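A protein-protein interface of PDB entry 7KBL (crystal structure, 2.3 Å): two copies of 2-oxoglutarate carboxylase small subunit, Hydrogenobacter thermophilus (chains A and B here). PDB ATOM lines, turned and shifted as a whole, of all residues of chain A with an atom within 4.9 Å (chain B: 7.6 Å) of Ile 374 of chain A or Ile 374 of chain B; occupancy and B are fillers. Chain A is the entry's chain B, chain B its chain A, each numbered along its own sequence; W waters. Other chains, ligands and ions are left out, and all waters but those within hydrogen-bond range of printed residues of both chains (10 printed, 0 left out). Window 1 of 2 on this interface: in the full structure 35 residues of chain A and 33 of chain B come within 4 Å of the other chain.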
ATOM      1  N   ARG A  28      22.575 -32.108  -1.347  1.00  0.00           N
ATOM      2  CA  ARG A  28      22.416 -30.867  -2.108  1.00  0.00           C
ATOM      3  C   ARG A  28      20.944 -30.565  -2.371  1.00  0.00           C
ATOM      4  O   ARG A  28      20.492 -29.438  -2.144  1.00  0.00           O
ATOM      5  CB  ARG A  28      23.205 -30.927  -3.425  1.00  0.00           C
ATOM      6  CG  ARG A  28      23.045 -29.674  -4.273  1.00  0.00           C
ATOM      7  CD  ARG A  28      24.075 -29.551  -5.391  1.00  0.00           C
ATOM      8  NE  ARG A  28      25.443 -29.745  -4.918  1.00  0.00           N
ATOM      9  CZ  ARG A  28      26.062 -28.957  -4.043  1.00  0.00           C
ATOM     10  NH1 ARG A  28      25.444 -27.896  -3.517  1.00  0.00           N
ATOM     11  NH2 ARG A  28      27.313 -29.227  -3.684  1.00  0.00           N
ATOM     12  N   PRO A 369      36.831 -31.285 -14.235  1.00  0.00           N
ATOM     13  CA  PRO A 369      36.410 -30.453 -15.372  1.00  0.00           C
ATOM     14  C   PRO A 369      35.142 -29.659 -15.133  1.00  0.00           C
ATOM     15  O   PRO A 369      34.225 -30.086 -14.425  1.00  0.00           O
ATOM     16  CB  PRO A 369      36.157 -31.467 -16.490  1.00  0.00           C
ATOM     17  CG  PRO A 369      36.660 -32.726 -16.051  1.00  0.00           C
ATOM     18  CD  PRO A 369      36.967 -32.696 -14.599  1.00  0.00           C
ATOM     19  N   GLY A 370      35.081 -28.499 -15.779  1.00  0.00           N
ATOM     20  CA  GLY A 370      33.844 -27.739 -15.826  1.00  0.00           C
ATOM     21  C   GLY A 370      33.708 -26.935 -17.111  1.00  0.00           C
ATOM     22  O   GLY A 370      34.682 -26.654 -17.821  1.00  0.00           O
ATOM     23  N   GLY A 371      32.485 -26.508 -17.361  1.00  0.00           N
ATOM     24  CA  GLY A 371      32.216 -25.647 -18.493  1.00  0.00           C
ATOM     25  C   GLY A 371      30.755 -25.695 -18.874  1.00  0.00           C
ATOM     26  O   GLY A 371      29.918 -26.273 -18.173  1.00  0.00           O
ATOM     27  N   PHE A 372      30.476 -25.053 -19.993  1.00  0.00           N
ATOM     28  CA  PHE A 372      29.158 -25.077 -20.607  1.00  0.00           C
ATOM     29  C   PHE A 372      28.814 -26.515 -20.983  1.00  0.00           C
ATOM     30  O   PHE A 372      29.580 -27.175 -21.680  1.00  0.00           O
ATOM     31  CB  PHE A 372      29.156 -24.169 -21.847  1.00  0.00           C
ATOM     32  CG  PHE A 372      27.781 -23.798 -22.363  1.00  0.00           C
ATOM     33  CD1 PHE A 372      26.726 -23.492 -21.486  1.00  0.00           C
ATOM     34  CD2 PHE A 372      27.554 -23.687 -23.724  1.00  0.00           C
ATOM     35  CE1 PHE A 372      25.461 -23.118 -21.987  1.00  0.00           C
ATOM     36  CE2 PHE A 372      26.294 -23.308 -24.229  1.00  0.00           C
ATOM     37  CZ  PHE A 372      25.266 -23.015 -23.374  1.00  0.00           C
ATOM     38  N   GLY A 373      27.688 -26.992 -20.488  1.00  0.00           N
ATOM     39  CA  GLY A 373      27.194 -28.316 -20.742  1.00  0.00           C
ATOM     40  C   GLY A 373      27.859 -29.417 -19.935  1.00  0.00           C
ATOM     41  O   GLY A 373      27.647 -30.593 -20.262  1.00  0.00           O
ATOM     42  N   ILE A 374      28.619 -29.080 -18.880  1.00  0.00           N
ATOM     43  CA  ILE A 374      29.328 -30.067 -18.069  1.00  0.00           C
ATOM     44  C   ILE A 374      28.784 -30.018 -16.652  1.00  0.00           C
ATOM     45  O   ILE A 374      28.644 -28.943 -16.061  1.00  0.00           O
ATOM     46  CB  ILE A 374      30.849 -29.849 -18.066  1.00  0.00           C
ATOM     47  CG1 ILE A 374      31.416 -30.027 -19.465  1.00  0.00           C
ATOM     48  CG2 ILE A 374      31.554 -30.830 -17.120  1.00  0.00           C
ATOM     49  CD1 ILE A 374      32.898 -29.714 -19.589  1.00  0.00           C
ATOM     50  N   ARG A 375      28.526 -31.194 -16.107  1.00  0.00           N
ATOM     51  CA  ARG A 375      28.039 -31.399 -14.752  1.00  0.00           C
ATOM     52  C   ARG A 375      28.848 -32.540 -14.146  1.00  0.00           C
ATOM     53  O   ARG A 375      29.117 -33.516 -14.837  1.00  0.00           O
ATOM     54  CB  ARG A 375      26.540 -31.721 -14.803  1.00  0.00           C
ATOM     55  CG  ARG A 375      25.957 -32.305 -13.522  1.00  0.00           C
ATOM     56  CD  ARG A 375      24.477 -32.500 -13.625  1.00  0.00           C
ATOM     57  NE  ARG A 375      23.945 -33.166 -12.446  1.00  0.00           N
ATOM     58  CZ  ARG A 375      22.681 -33.548 -12.306  1.00  0.00           C
ATOM     59  NH1 ARG A 375      21.805 -33.319 -13.291  1.00  0.00           N
ATOM     60  NH2 ARG A 375      22.287 -34.135 -11.178  1.00  0.00           N
ATOM     61  N   VAL A 376      29.254 -32.412 -12.874  1.00  0.00           N
ATOM     62  CA  VAL A 376      30.047 -33.429 -12.176  1.00  0.00           C
ATOM     63  C   VAL A 376      29.347 -33.835 -10.885  1.00  0.00           C
ATOM     64  O   VAL A 376      28.998 -32.985 -10.060  1.00  0.00           O
ATOM     65  CB  VAL A 376      31.475 -32.960 -11.864  1.00  0.00           C
ATOM     66  CG1 VAL A 376      32.288 -34.101 -11.140  1.00  0.00           C
ATOM     67  CG2 VAL A 376      32.176 -32.540 -13.111  1.00  0.00           C
ATOM     68  N   LEU A 397      30.660 -38.168 -14.644  1.00  0.00           N
ATOM     69  CA  LEU A 397      30.870 -37.018 -15.507  1.00  0.00           C
ATOM     70  C   LEU A 397      29.738 -37.010 -16.517  1.00  0.00           C
ATOM     71  O   LEU A 397      29.555 -38.004 -17.235  1.00  0.00           O
ATOM     72  CB  LEU A 397      32.218 -37.107 -16.219  1.00  0.00           C
ATOM     73  CG  LEU A 397      32.532 -35.993 -17.205  1.00  0.00           C
ATOM     74  CD1 LEU A 397      32.608 -34.646 -16.442  1.00  0.00           C
ATOM     75  CD2 LEU A 397      33.828 -36.323 -17.973  1.00  0.00           C
ATOM     76  N   ILE A 398      28.982 -35.913 -16.545  1.00  0.00           N
ATOM     77  CA  ILE A 398      27.794 -35.787 -17.373  1.00  0.00           C
ATOM     78  C   ILE A 398      27.921 -34.557 -18.276  1.00  0.00           C
ATOM     79  O   ILE A 398      28.351 -33.487 -17.838  1.00  0.00           O
ATOM     80  CB  ILE A 398      26.514 -35.702 -16.516  1.00  0.00           C
ATOM     81  CG1 ILE A 398      26.405 -36.912 -15.604  1.00  0.00           C
ATOM     82  CG2 ILE A 398      25.247 -35.627 -17.376  1.00  0.00           C
ATOM     83  CD1 ILE A 398      26.511 -36.529 -14.137  1.00  0.00           C
ATOM     84  N   VAL A 399      27.530 -34.706 -19.537  1.00  0.00           N
ATOM     85  CA  VAL A 399      27.500 -33.593 -20.469  1.00  0.00           C
ATOM     86  C   VAL A 399      26.141 -33.543 -21.140  1.00  0.00           C
ATOM     87  O   VAL A 399      25.413 -34.534 -21.206  1.00  0.00           O
ATOM     88  CB  VAL A 399      28.620 -33.651 -21.547  1.00  0.00           C
ATOM     89  CG1 VAL A 399      29.958 -33.838 -20.926  1.00  0.00           C
ATOM     90  CG2 VAL A 399      28.365 -34.779 -22.561  1.00  0.00           C
ATOM     91  N   ARG A 410      32.069 -33.044 -26.593  1.00  0.00           N
ATOM     92  CA  ARG A 410      32.137 -32.414 -25.274  1.00  0.00           C
ATOM     93  C   ARG A 410      32.531 -33.412 -24.179  1.00  0.00           C
ATOM     94  O   ARG A 410      33.350 -33.090 -23.310  1.00  0.00           O
ATOM     95  CB  ARG A 410      30.793 -31.780 -24.958  1.00  0.00           C
ATOM     96  CG  ARG A 410      30.656 -31.200 -23.564  1.00  0.00           C
ATOM     97  CD  ARG A 410      29.497 -30.169 -23.563  1.00  0.00           C
ATOM     98  NE  ARG A 410      29.858 -29.015 -24.347  1.00  0.00           N
ATOM     99  CZ  ARG A 410      29.014 -28.194 -24.962  1.00  0.00           C
ATOM    100  NH1 ARG A 410      27.696 -28.372 -24.887  1.00  0.00           N
ATOM    101  NH2 ARG A 410      29.529 -27.168 -25.648  1.00  0.00           N
ATOM    102  N   ALA A 414      35.974 -33.211 -22.153  1.00  0.00           N
ATOM    103  CA  ALA A 414      35.930 -33.177 -20.696  1.00  0.00           C
ATOM    104  C   ALA A 414      36.791 -34.290 -20.097  1.00  0.00           C
ATOM    105  O   ALA A 414      37.623 -34.029 -19.229  1.00  0.00           O
ATOM    106  CB  ALA A 414      34.488 -33.267 -20.225  1.00  0.00           C
ATOM    107  N   ARG B  28      38.922 -25.377 -23.897  1.00  0.00           N
ATOM    108  CA  ARG B  28      37.816 -26.324 -23.959  1.00  0.00           C
ATOM    109  C   ARG B  28      36.965 -26.081 -25.210  1.00  0.00           C
ATOM    110  O   ARG B  28      36.628 -27.027 -25.939  1.00  0.00           O
ATOM    111  CB  ARG B  28      36.962 -26.258 -22.688  1.00  0.00           C
ATOM    112  CG  ARG B  28      35.780 -27.236 -22.752  1.00  0.00           C
ATOM    113  CD  ARG B  28      35.025 -27.529 -21.417  1.00  0.00           C
ATOM    114  NE  ARG B  28      35.943 -27.840 -20.342  1.00  0.00           N
ATOM    115  CZ  ARG B  28      36.699 -28.916 -20.276  1.00  0.00           C
ATOM    116  NH1 ARG B  28      36.656 -29.852 -21.226  1.00  0.00           N
ATOM    117  NH2 ARG B  28      37.523 -29.015 -19.254  1.00  0.00           N
ATOM    118  N   GLU B  32      36.520 -28.944 -28.211  1.00  0.00           N
ATOM    119  CA  GLU B  32      35.204 -29.333 -28.696  1.00  0.00           C
ATOM    120  C   GLU B  32      35.075 -29.085 -30.191  1.00  0.00           C
ATOM    121  O   GLU B  32      34.466 -29.889 -30.902  1.00  0.00           O
ATOM    122  CB  GLU B  32      34.112 -28.586 -27.918  1.00  0.00           C
ATOM    123  CG  GLU B  32      33.967 -29.051 -26.435  1.00  0.00           C
ATOM    124  CD  GLU B  32      32.827 -28.363 -25.667  1.00  0.00           C
ATOM    125  OE1 GLU B  32      32.081 -27.530 -26.270  1.00  0.00           O
ATOM    126  OE2 GLU B  32      32.710 -28.625 -24.442  1.00  0.00           O
ATOM    127  N   MET B 310      24.096 -19.283 -19.763  1.00  0.00           N
ATOM    128  CA  MET B 310      23.168 -20.186 -19.105  1.00  0.00           C
ATOM    129  C   MET B 310      21.739 -19.835 -19.467  1.00  0.00           C
ATOM    130  O   MET B 310      20.903 -20.727 -19.631  1.00  0.00           O
ATOM    131  CB  MET B 310      23.359 -20.153 -17.585  1.00  0.00           C
ATOM    132  CG  MET B 310      24.719 -20.532 -17.147  1.00  0.00           C
ATOM    133  SD  MET B 310      25.173 -22.196 -17.682  1.00  0.00           S
ATOM    134  CE  MET B 310      24.437 -23.042 -16.285  1.00  0.00           C
ATOM    135  N   VAL B 368      35.395 -29.185  -5.328  1.00  0.00           N
ATOM    136  CA  VAL B 368      34.542 -28.469  -6.279  1.00  0.00           C
ATOM    137  C   VAL B 368      33.132 -29.030  -6.148  1.00  0.00           C
ATOM    138  O   VAL B 368      32.946 -30.243  -6.315  1.00  0.00           O
ATOM    139  CB  VAL B 368      35.033 -28.629  -7.722  1.00  0.00           C
ATOM    140  CG1 VAL B 368      34.159 -27.790  -8.738  1.00  0.00           C
ATOM    141  CG2 VAL B 368      36.479 -28.231  -7.814  1.00  0.00           C
ATOM    142  N   PRO B 369      32.140 -28.211  -5.877  1.00  0.00           N
ATOM    143  CA  PRO B 369      30.777 -28.696  -5.918  1.00  0.00           C
ATOM    144  C   PRO B 369      30.299 -28.932  -7.349  1.00  0.00           C
ATOM    145  O   PRO B 369      30.702 -28.250  -8.304  1.00  0.00           O
ATOM    146  CB  PRO B 369      29.993 -27.568  -5.253  1.00  0.00           C
ATOM    147  CG  PRO B 369      30.798 -26.383  -5.448  1.00  0.00           C
ATOM    148  CD  PRO B 369      32.208 -26.787  -5.522  1.00  0.00           C
ATOM    149  N   GLY B 370      29.377 -29.882  -7.471  1.00  0.00           N
ATOM    150  CA  GLY B 370      28.712 -30.125  -8.722  1.00  0.00           C
ATOM    151  C   GLY B 370      27.276 -30.525  -8.469  1.00  0.00           C
ATOM    152  O   GLY B 370      26.857 -30.783  -7.341  1.00  0.00           O
ATOM    153  N   GLY B 371      26.513 -30.527  -9.540  1.00  0.00           N
ATOM    154  CA  GLY B 371      25.138 -30.947  -9.442  1.00  0.00           C
ATOM    155  C   GLY B 371      24.316 -30.357 -10.563  1.00  0.00           C
ATOM    156  O   GLY B 371      24.831 -29.709 -11.474  1.00  0.00           O
ATOM    157  N   PHE B 372      23.021 -30.589 -10.433  1.00  0.00           N
ATOM    158  CA  PHE B 372      22.008 -30.030 -11.300  1.00  0.00           C
ATOM    159  C   PHE B 372      22.034 -28.502 -11.243  1.00  0.00           C
ATOM    160  O   PHE B 372      21.906 -27.906 -10.171  1.00  0.00           O
ATOM    161  CB  PHE B 372      20.664 -30.598 -10.847  1.00  0.00           C
ATOM    162  CG  PHE B 372      19.472 -30.247 -11.737  1.00  0.00           C
ATOM    163  CD1 PHE B 372      18.763 -29.085 -11.530  1.00  0.00           C
ATOM    164  CD2 PHE B 372      19.055 -31.096 -12.731  1.00  0.00           C
ATOM    165  CE1 PHE B 372      17.664 -28.769 -12.324  1.00  0.00           C
ATOM    166  CE2 PHE B 372      17.953 -30.795 -13.535  1.00  0.00           C
ATOM    167  CZ  PHE B 372      17.253 -29.652 -13.323  1.00  0.00           C
ATOM    168  N   GLY B 373      22.213 -27.864 -12.400  1.00  0.00           N
ATOM    169  CA  GLY B 373      22.190 -26.422 -12.444  1.00  0.00           C
ATOM    170  C   GLY B 373      23.447 -25.769 -11.945  1.00  0.00           C
ATOM    171  O   GLY B 373      23.422 -24.595 -11.588  1.00  0.00           O
ATOM    172  N   ILE B 374      24.530 -26.515 -11.837  1.00  0.00           N
ATOM    173  CA  ILE B 374      25.796 -26.005 -11.342  1.00  0.00           C
ATOM    174  C   ILE B 374      26.853 -26.138 -12.424  1.00  0.00           C
ATOM    175  O   ILE B 374      26.985 -27.179 -13.067  1.00  0.00           O
ATOM    176  CB  ILE B 374      26.249 -26.730 -10.056  1.00  0.00           C
ATOM    177  CG1 ILE B 374      25.266 -26.457  -8.929  1.00  0.00           C
ATOM    178  CG2 ILE B 374      27.623 -26.252  -9.661  1.00  0.00           C
ATOM    179  CD1 ILE B 374      25.548 -27.250  -7.652  1.00  0.00           C
ATOM    180  N   ARG B 375      27.651 -25.099 -12.557  1.00  0.00           N
ATOM    181  CA  ARG B 375      28.740 -25.007 -13.512  1.00  0.00           C
ATOM    182  C   ARG B 375      29.927 -24.380 -12.802  1.00  0.00           C
ATOM    183  O   ARG B 375      29.744 -23.473 -11.985  1.00  0.00           O
ATOM    184  CB  ARG B 375      28.331 -24.160 -14.747  1.00  0.00           C
ATOM    185  CG  ARG B 375      29.477 -23.697 -15.664  1.00  0.00           C
ATOM    186  CD  ARG B 375      28.963 -23.016 -16.952  1.00  0.00           C
ATOM    187  NE  ARG B 375      30.083 -22.521 -17.761  1.00  0.00           N
ATOM    188  CZ  ARG B 375      29.950 -21.793 -18.854  1.00  0.00           C
ATOM    189  NH1 ARG B 375      28.744 -21.471 -19.270  1.00  0.00           N
ATOM    190  NH2 ARG B 375      31.020 -21.389 -19.539  1.00  0.00           N
ATOM    191  N   VAL B 376      31.128 -24.869 -13.096  1.00  0.00           N
ATOM    192  CA  VAL B 376      32.332 -24.333 -12.489  1.00  0.00           C
ATOM    193  C   VAL B 376      33.353 -23.979 -13.559  1.00  0.00           C
ATOM    194  O   VAL B 376      33.692 -24.813 -14.409  1.00  0.00           O
ATOM    195  CB  VAL B 376      32.959 -25.288 -11.458  1.00  0.00           C
ATOM    196  CG1 VAL B 376      34.140 -24.623 -10.877  1.00  0.00           C
ATOM    197  CG2 VAL B 376      31.940 -25.636 -10.395  1.00  0.00           C
ATOM    198  N   GLU B 377      33.884 -22.751 -13.470  1.00  0.00           N
ATOM    199  CA  GLU B 377      34.965 -22.271 -14.321  1.00  0.00           C
ATOM    200  C   GLU B 377      36.185 -22.088 -13.429  1.00  0.00           C
ATOM    201  O   GLU B 377      36.205 -21.171 -12.607  1.00  0.00           O
ATOM    202  CB  GLU B 377      34.582 -20.959 -14.988  1.00  0.00           C
ATOM    203  CG  GLU B 377      33.403 -21.018 -15.964  1.00  0.00           C
ATOM    204  CD  GLU B 377      33.773 -21.773 -17.238  1.00  0.00           C
ATOM    205  OE1 GLU B 377      34.965 -21.748 -17.630  1.00  0.00           O
ATOM    206  OE2 GLU B 377      32.891 -22.409 -17.831  1.00  0.00           O
ATOM    207  N   LEU B 397      31.894 -19.650  -9.797  1.00  0.00           N
ATOM    208  CA  LEU B 397      30.844 -20.598  -9.527  1.00  0.00           C
ATOM    209  C   LEU B 397      29.577 -20.035 -10.132  1.00  0.00           C
ATOM    210  O   LEU B 397      29.207 -18.910  -9.817  1.00  0.00           O
ATOM    211  CB  LEU B 397      30.714 -20.816  -8.031  1.00  0.00           C
ATOM    212  CG  LEU B 397      29.619 -21.719  -7.559  1.00  0.00           C
ATOM    213  CD1 LEU B 397      29.827 -23.156  -8.078  1.00  0.00           C
ATOM    214  CD2 LEU B 397      29.672 -21.619  -6.040  1.00  0.00           C
ATOM    215  N   ILE B 398      28.959 -20.794 -11.036  1.00  0.00           N
ATOM    216  CA  ILE B 398      27.790 -20.357 -11.786  1.00  0.00           C
ATOM    217  C   ILE B 398      26.649 -21.328 -11.554  1.00  0.00           C
ATOM    218  O   ILE B 398      26.820 -22.541 -11.673  1.00  0.00           O
ATOM    219  CB  ILE B 398      28.107 -20.251 -13.291  1.00  0.00           C
ATOM    220  CG1 ILE B 398      29.293 -19.301 -13.512  1.00  0.00           C
ATOM    221  CG2 ILE B 398      26.909 -19.751 -14.107  1.00  0.00           C
ATOM    222  CD1 ILE B 398      30.383 -19.926 -14.283  1.00  0.00           C
ATOM    223  N   VAL B 399      25.472 -20.798 -11.296  1.00  0.00           N
ATOM    224  CA  VAL B 399      24.288 -21.623 -11.192  1.00  0.00           C
ATOM    225  C   VAL B 399      23.210 -21.019 -12.078  1.00  0.00           C
ATOM    226  O   VAL B 399      23.255 -19.843 -12.464  1.00  0.00           O
ATOM    227  CB  VAL B 399      23.761 -21.772  -9.752  1.00  0.00           C
ATOM    228  CG1 VAL B 399      24.904 -22.099  -8.794  1.00  0.00           C
ATOM    229  CG2 VAL B 399      23.015 -20.549  -9.314  1.00  0.00           C
ATOM    230  N   TRP B 400      22.221 -21.872 -12.352  1.00  0.00           N
ATOM    231  CA  TRP B 400      21.022 -21.569 -13.097  1.00  0.00           C
ATOM    232  C   TRP B 400      19.833 -22.248 -12.438  1.00  0.00           C
ATOM    233  O   TRP B 400      19.937 -23.395 -12.008  1.00  0.00           O
ATOM    234  CB  TRP B 400      21.148 -22.072 -14.532  1.00  0.00           C
ATOM    235  CG  TRP B 400      19.944 -21.826 -15.329  1.00  0.00           C
ATOM    236  CD1 TRP B 400      19.661 -20.678 -16.043  1.00  0.00           C
ATOM    237  CD2 TRP B 400      18.855 -22.705 -15.544  1.00  0.00           C
ATOM    238  NE1 TRP B 400      18.477 -20.809 -16.693  1.00  0.00           N
ATOM    239  CE2 TRP B 400      17.945 -22.037 -16.402  1.00  0.00           C
ATOM    240  CE3 TRP B 400      18.548 -23.998 -15.114  1.00  0.00           C
ATOM    241  CZ2 TRP B 400      16.753 -22.617 -16.818  1.00  0.00           C
ATOM    242  CZ3 TRP B 400      17.369 -24.573 -15.535  1.00  0.00           C
ATOM    243  CH2 TRP B 400      16.480 -23.883 -16.374  1.00  0.00           C
ATOM    244  N   ARG B 410      20.304 -22.301  -4.746  1.00  0.00           N
ATOM    245  CA  ARG B 410      21.281 -23.196  -5.363  1.00  0.00           C
ATOM    246  C   ARG B 410      22.690 -22.642  -5.238  1.00  0.00           C
ATOM    247  O   ARG B 410      23.638 -23.409  -5.025  1.00  0.00           O
ATOM    248  CB  ARG B 410      20.923 -23.452  -6.833  1.00  0.00           C
ATOM    249  CG  ARG B 410      21.916 -24.333  -7.620  1.00  0.00           C
ATOM    250  CD  ARG B 410      21.249 -24.867  -8.914  1.00  0.00           C
ATOM    251  NE  ARG B 410      20.224 -25.828  -8.580  1.00  0.00           N
ATOM    252  CZ  ARG B 410      19.143 -26.078  -9.289  1.00  0.00           C
ATOM    253  NH1 ARG B 410      18.908 -25.431 -10.423  1.00  0.00           N
ATOM    254  NH2 ARG B 410      18.295 -27.007  -8.845  1.00  0.00           N
ATOM    255  N   MET B 411      22.854 -21.318  -5.401  1.00  0.00           N
ATOM    256  CA  MET B 411      24.161 -20.721  -5.176  1.00  0.00           C
ATOM    257  C   MET B 411      24.555 -20.781  -3.713  1.00  0.00           C
ATOM    258  O   MET B 411      25.721 -21.037  -3.389  1.00  0.00           O
ATOM    259  CB  MET B 411      24.188 -19.269  -5.611  1.00  0.00           C
ATOM    260  CG  MET B 411      25.493 -18.625  -5.366  1.00  0.00           C
ATOM    261  SD  MET B 411      26.832 -19.339  -6.304  1.00  0.00           S
ATOM    262  CE  MET B 411      26.344 -18.892  -7.974  1.00  0.00           C
ATOM    263  N   SER B 413      23.665 -23.001  -1.592  1.00  0.00           N
ATOM    264  CA  SER B 413      24.007 -24.381  -1.280  1.00  0.00           C
ATOM    265  C   SER B 413      25.289 -24.832  -1.972  1.00  0.00           C
ATOM    266  O   SER B 413      26.019 -25.659  -1.410  1.00  0.00           O
ATOM    267  CB  SER B 413      22.851 -25.303  -1.646  1.00  0.00           C
ATOM    268  OG  SER B 413      21.697 -24.960  -0.898  1.00  0.00           O
ATOM    269  N   ALA B 414      25.599 -24.295  -3.163  1.00  0.00           N
ATOM    270  CA  ALA B 414      26.869 -24.613  -3.816  1.00  0.00           C
ATOM    271  C   ALA B 414      28.034 -23.995  -3.057  1.00  0.00           C
ATOM    272  O   ALA B 414      29.015 -24.675  -2.748  1.00  0.00           O
ATOM    273  CB  ALA B 414      26.871 -24.169  -5.282  1.00  0.00           C
ATOM    274  N   LEU B 415      27.924 -22.706  -2.724  1.00  0.00           N
ATOM    275  CA  LEU B 415      28.943 -22.010  -1.930  1.00  0.00           C
ATOM    276  C   LEU B 415      29.202 -22.691  -0.590  1.00  0.00           C
ATOM    277  O   LEU B 415      30.349 -22.743  -0.128  1.00  0.00           O
ATOM    278  CB  LEU B 415      28.502 -20.566  -1.671  1.00  0.00           C
ATOM    279  CG  LEU B 415      28.512 -19.550  -2.821  1.00  0.00           C
ATOM    280  CD1 LEU B 415      27.721 -18.332  -2.471  1.00  0.00           C
ATOM    281  CD2 LEU B 415      29.912 -19.158  -3.135  1.00  0.00           C
ATOM    282  N   THR B 417      29.194 -25.726   0.120  1.00  0.00           N
ATOM    283  CA  THR B 417      29.903 -26.991  -0.030  1.00  0.00           C
ATOM    284  C   THR B 417      31.219 -26.830  -0.758  1.00  0.00           C
ATOM    285  O   THR B 417      31.941 -27.821  -0.926  1.00  0.00           O
ATOM    286  CB  THR B 417      29.036 -28.005  -0.760  1.00  0.00           C
ATOM    287  OG1 THR B 417      28.811 -27.581  -2.116  1.00  0.00           O
ATOM    288  CG2 THR B 417      27.698 -28.135  -0.041  1.00  0.00           C
ATOM    289  N   TYR B 418      31.535 -25.613  -1.207  1.00  0.00           N
ATOM    290  CA  TYR B 418      32.788 -25.329  -1.903  1.00  0.00           C
ATOM    291  C   TYR B 418      33.885 -25.093  -0.859  1.00  0.00           C
ATOM    292  O   TYR B 418      33.987 -24.007  -0.274  1.00  0.00           O
ATOM    293  CB  TYR B 418      32.613 -24.125  -2.832  1.00  0.00           C
ATOM    294  CG  TYR B 418      33.520 -24.094  -4.035  1.00  0.00           C
ATOM    295  CD1 TYR B 418      34.800 -24.605  -3.990  1.00  0.00           C
ATOM    296  CD2 TYR B 418      33.081 -23.541  -5.230  1.00  0.00           C
ATOM    297  CE1 TYR B 418      35.618 -24.595  -5.106  1.00  0.00           C
ATOM    298  CE2 TYR B 418      33.889 -23.488  -6.349  1.00  0.00           C
ATOM    299  CZ  TYR B 418      35.156 -24.015  -6.295  1.00  0.00           C
ATOM    300  OH  TYR B 418      35.952 -23.970  -7.435  1.00  0.00           O
HETATM  301  O   HOH W   1      28.100 -29.772 -11.832  1.00  0.00           O
HETATM  302  O   HOH W   2      34.381 -30.302 -22.960  1.00  0.00           O
HETATM  303  O   HOH W   3      31.965 -26.444 -22.781  1.00  0.00           O
HETATM  304  O   HOH W   4      37.810 -27.154 -17.154  1.00  0.00           O
HETATM  305  O   HOH W   5      30.689 -27.307 -14.920  1.00  0.00           O
HETATM  306  O   HOH W   6      35.094 -24.145 -19.488  1.00  0.00           O
HETATM  307  O   HOH W   7      28.586 -31.523  -4.933  1.00  0.00           O
HETATM  308  O   HOH W   8      36.027 -25.131 -15.119  1.00  0.00           O
HETATM  309  O   HOH W   9      23.402 -26.350  -4.837  1.00  0.00           O
HETATM  310  O   HOH W  10      29.399 -33.154  -7.180  1.00  0.00           O
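NE of Arg 28 of chain B lies within hydrogen-bond range of O of Gly 370 of chain A, 3.1 Å away. The guanidinium group of Arg 410 of chain A lies within salt-bridge range of the side-chain carboxylate of Glu 32 of chain B (2.7 Å). NE of Arg 28 of chain A lies within hydrogen-bond range of O of Gly 370 of chain B (3.0 Å). O of Ser 413 of chain B is in hydrogen-bond range of NH1 of Arg 28 of chain A. The side-chain hydroxyl of Thr 417 of chain B lies within hydrogen-bond range of the guanidinium group of Arg 28 of chain A. The backbone NH of Phe 372 of chain A sits close to the guanidinium group of Arg 375 of chain B, at 3.4 Å. N of Phe 372 of chain B lies close to NE of Arg 375 of chain A, 3.4 Å away.
OE2 of Glu 377 of chain B is in salt-bridge range of NH2 of Arg 375 of chain B (2.7 Å). O of Ile 398 of chain A sits at hydrogen-bond distance from N of Arg 375 of chain A (2.9 Å).
Ile 374 of chain A touches two residues of chain B. Of the printed residues of chain B, Ala 414 of chain A touches Arg 28. Printed residues of chain A within 4 Å of Arg 28 of chain B: Pro 369, Gly 370, Ile 374 and Ala 414. Ile 374 of chain B touches two residues of chain A. Met 411 of chain B touches none of the printed residues of chain A. The nearest residue of chain B that does not touch Ile 374 of chain A is Arg 375 of chain B (4.7 Å).
Hydrophobic or aromatic side chains of chain B within 4 Å of the printed part of chain A: Pro 369, Phe 372 and Ile 374. Printed residues of chain A that touch a printed residue of chain B: Arg 28, Pro 369, Gly 370, Gly 371, Phe 372, Ile 374, Arg 375, Val 376, Arg 410 and Ala 414. Hydrophobic or aromatic side chains of chain A that line the printed part of chain B: Pro 369, Phe 372 and Ile 374. Among the printed residues, 21 pairs touch across the chains. Among the printed residues, Asp or Glu carboxylates within 4 Å of a Lys or Arg side-chain nitrogen of the other chain: Arg 410 of chain A with Glu 32 of chain B.
Gly 371 of chain A touches Val 376 of chain B, and with the chains exchanged Val 376 of chain A touches Gly 371 of chain B. Phe 372 of chain A touches Arg 375 of chain B, and with the chains exchanged Arg 375 of chain A touches Phe 372 of chain B.
Water W1 lies within hydrogen-bond range of the backbone NH of Gly 371 of chain B (2.9 Å), the backbone NH of Val 376 of chain A (3.1 Å) and the backbone carbonyl oxygen of Ile 374 of chain B (3.1 Å).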
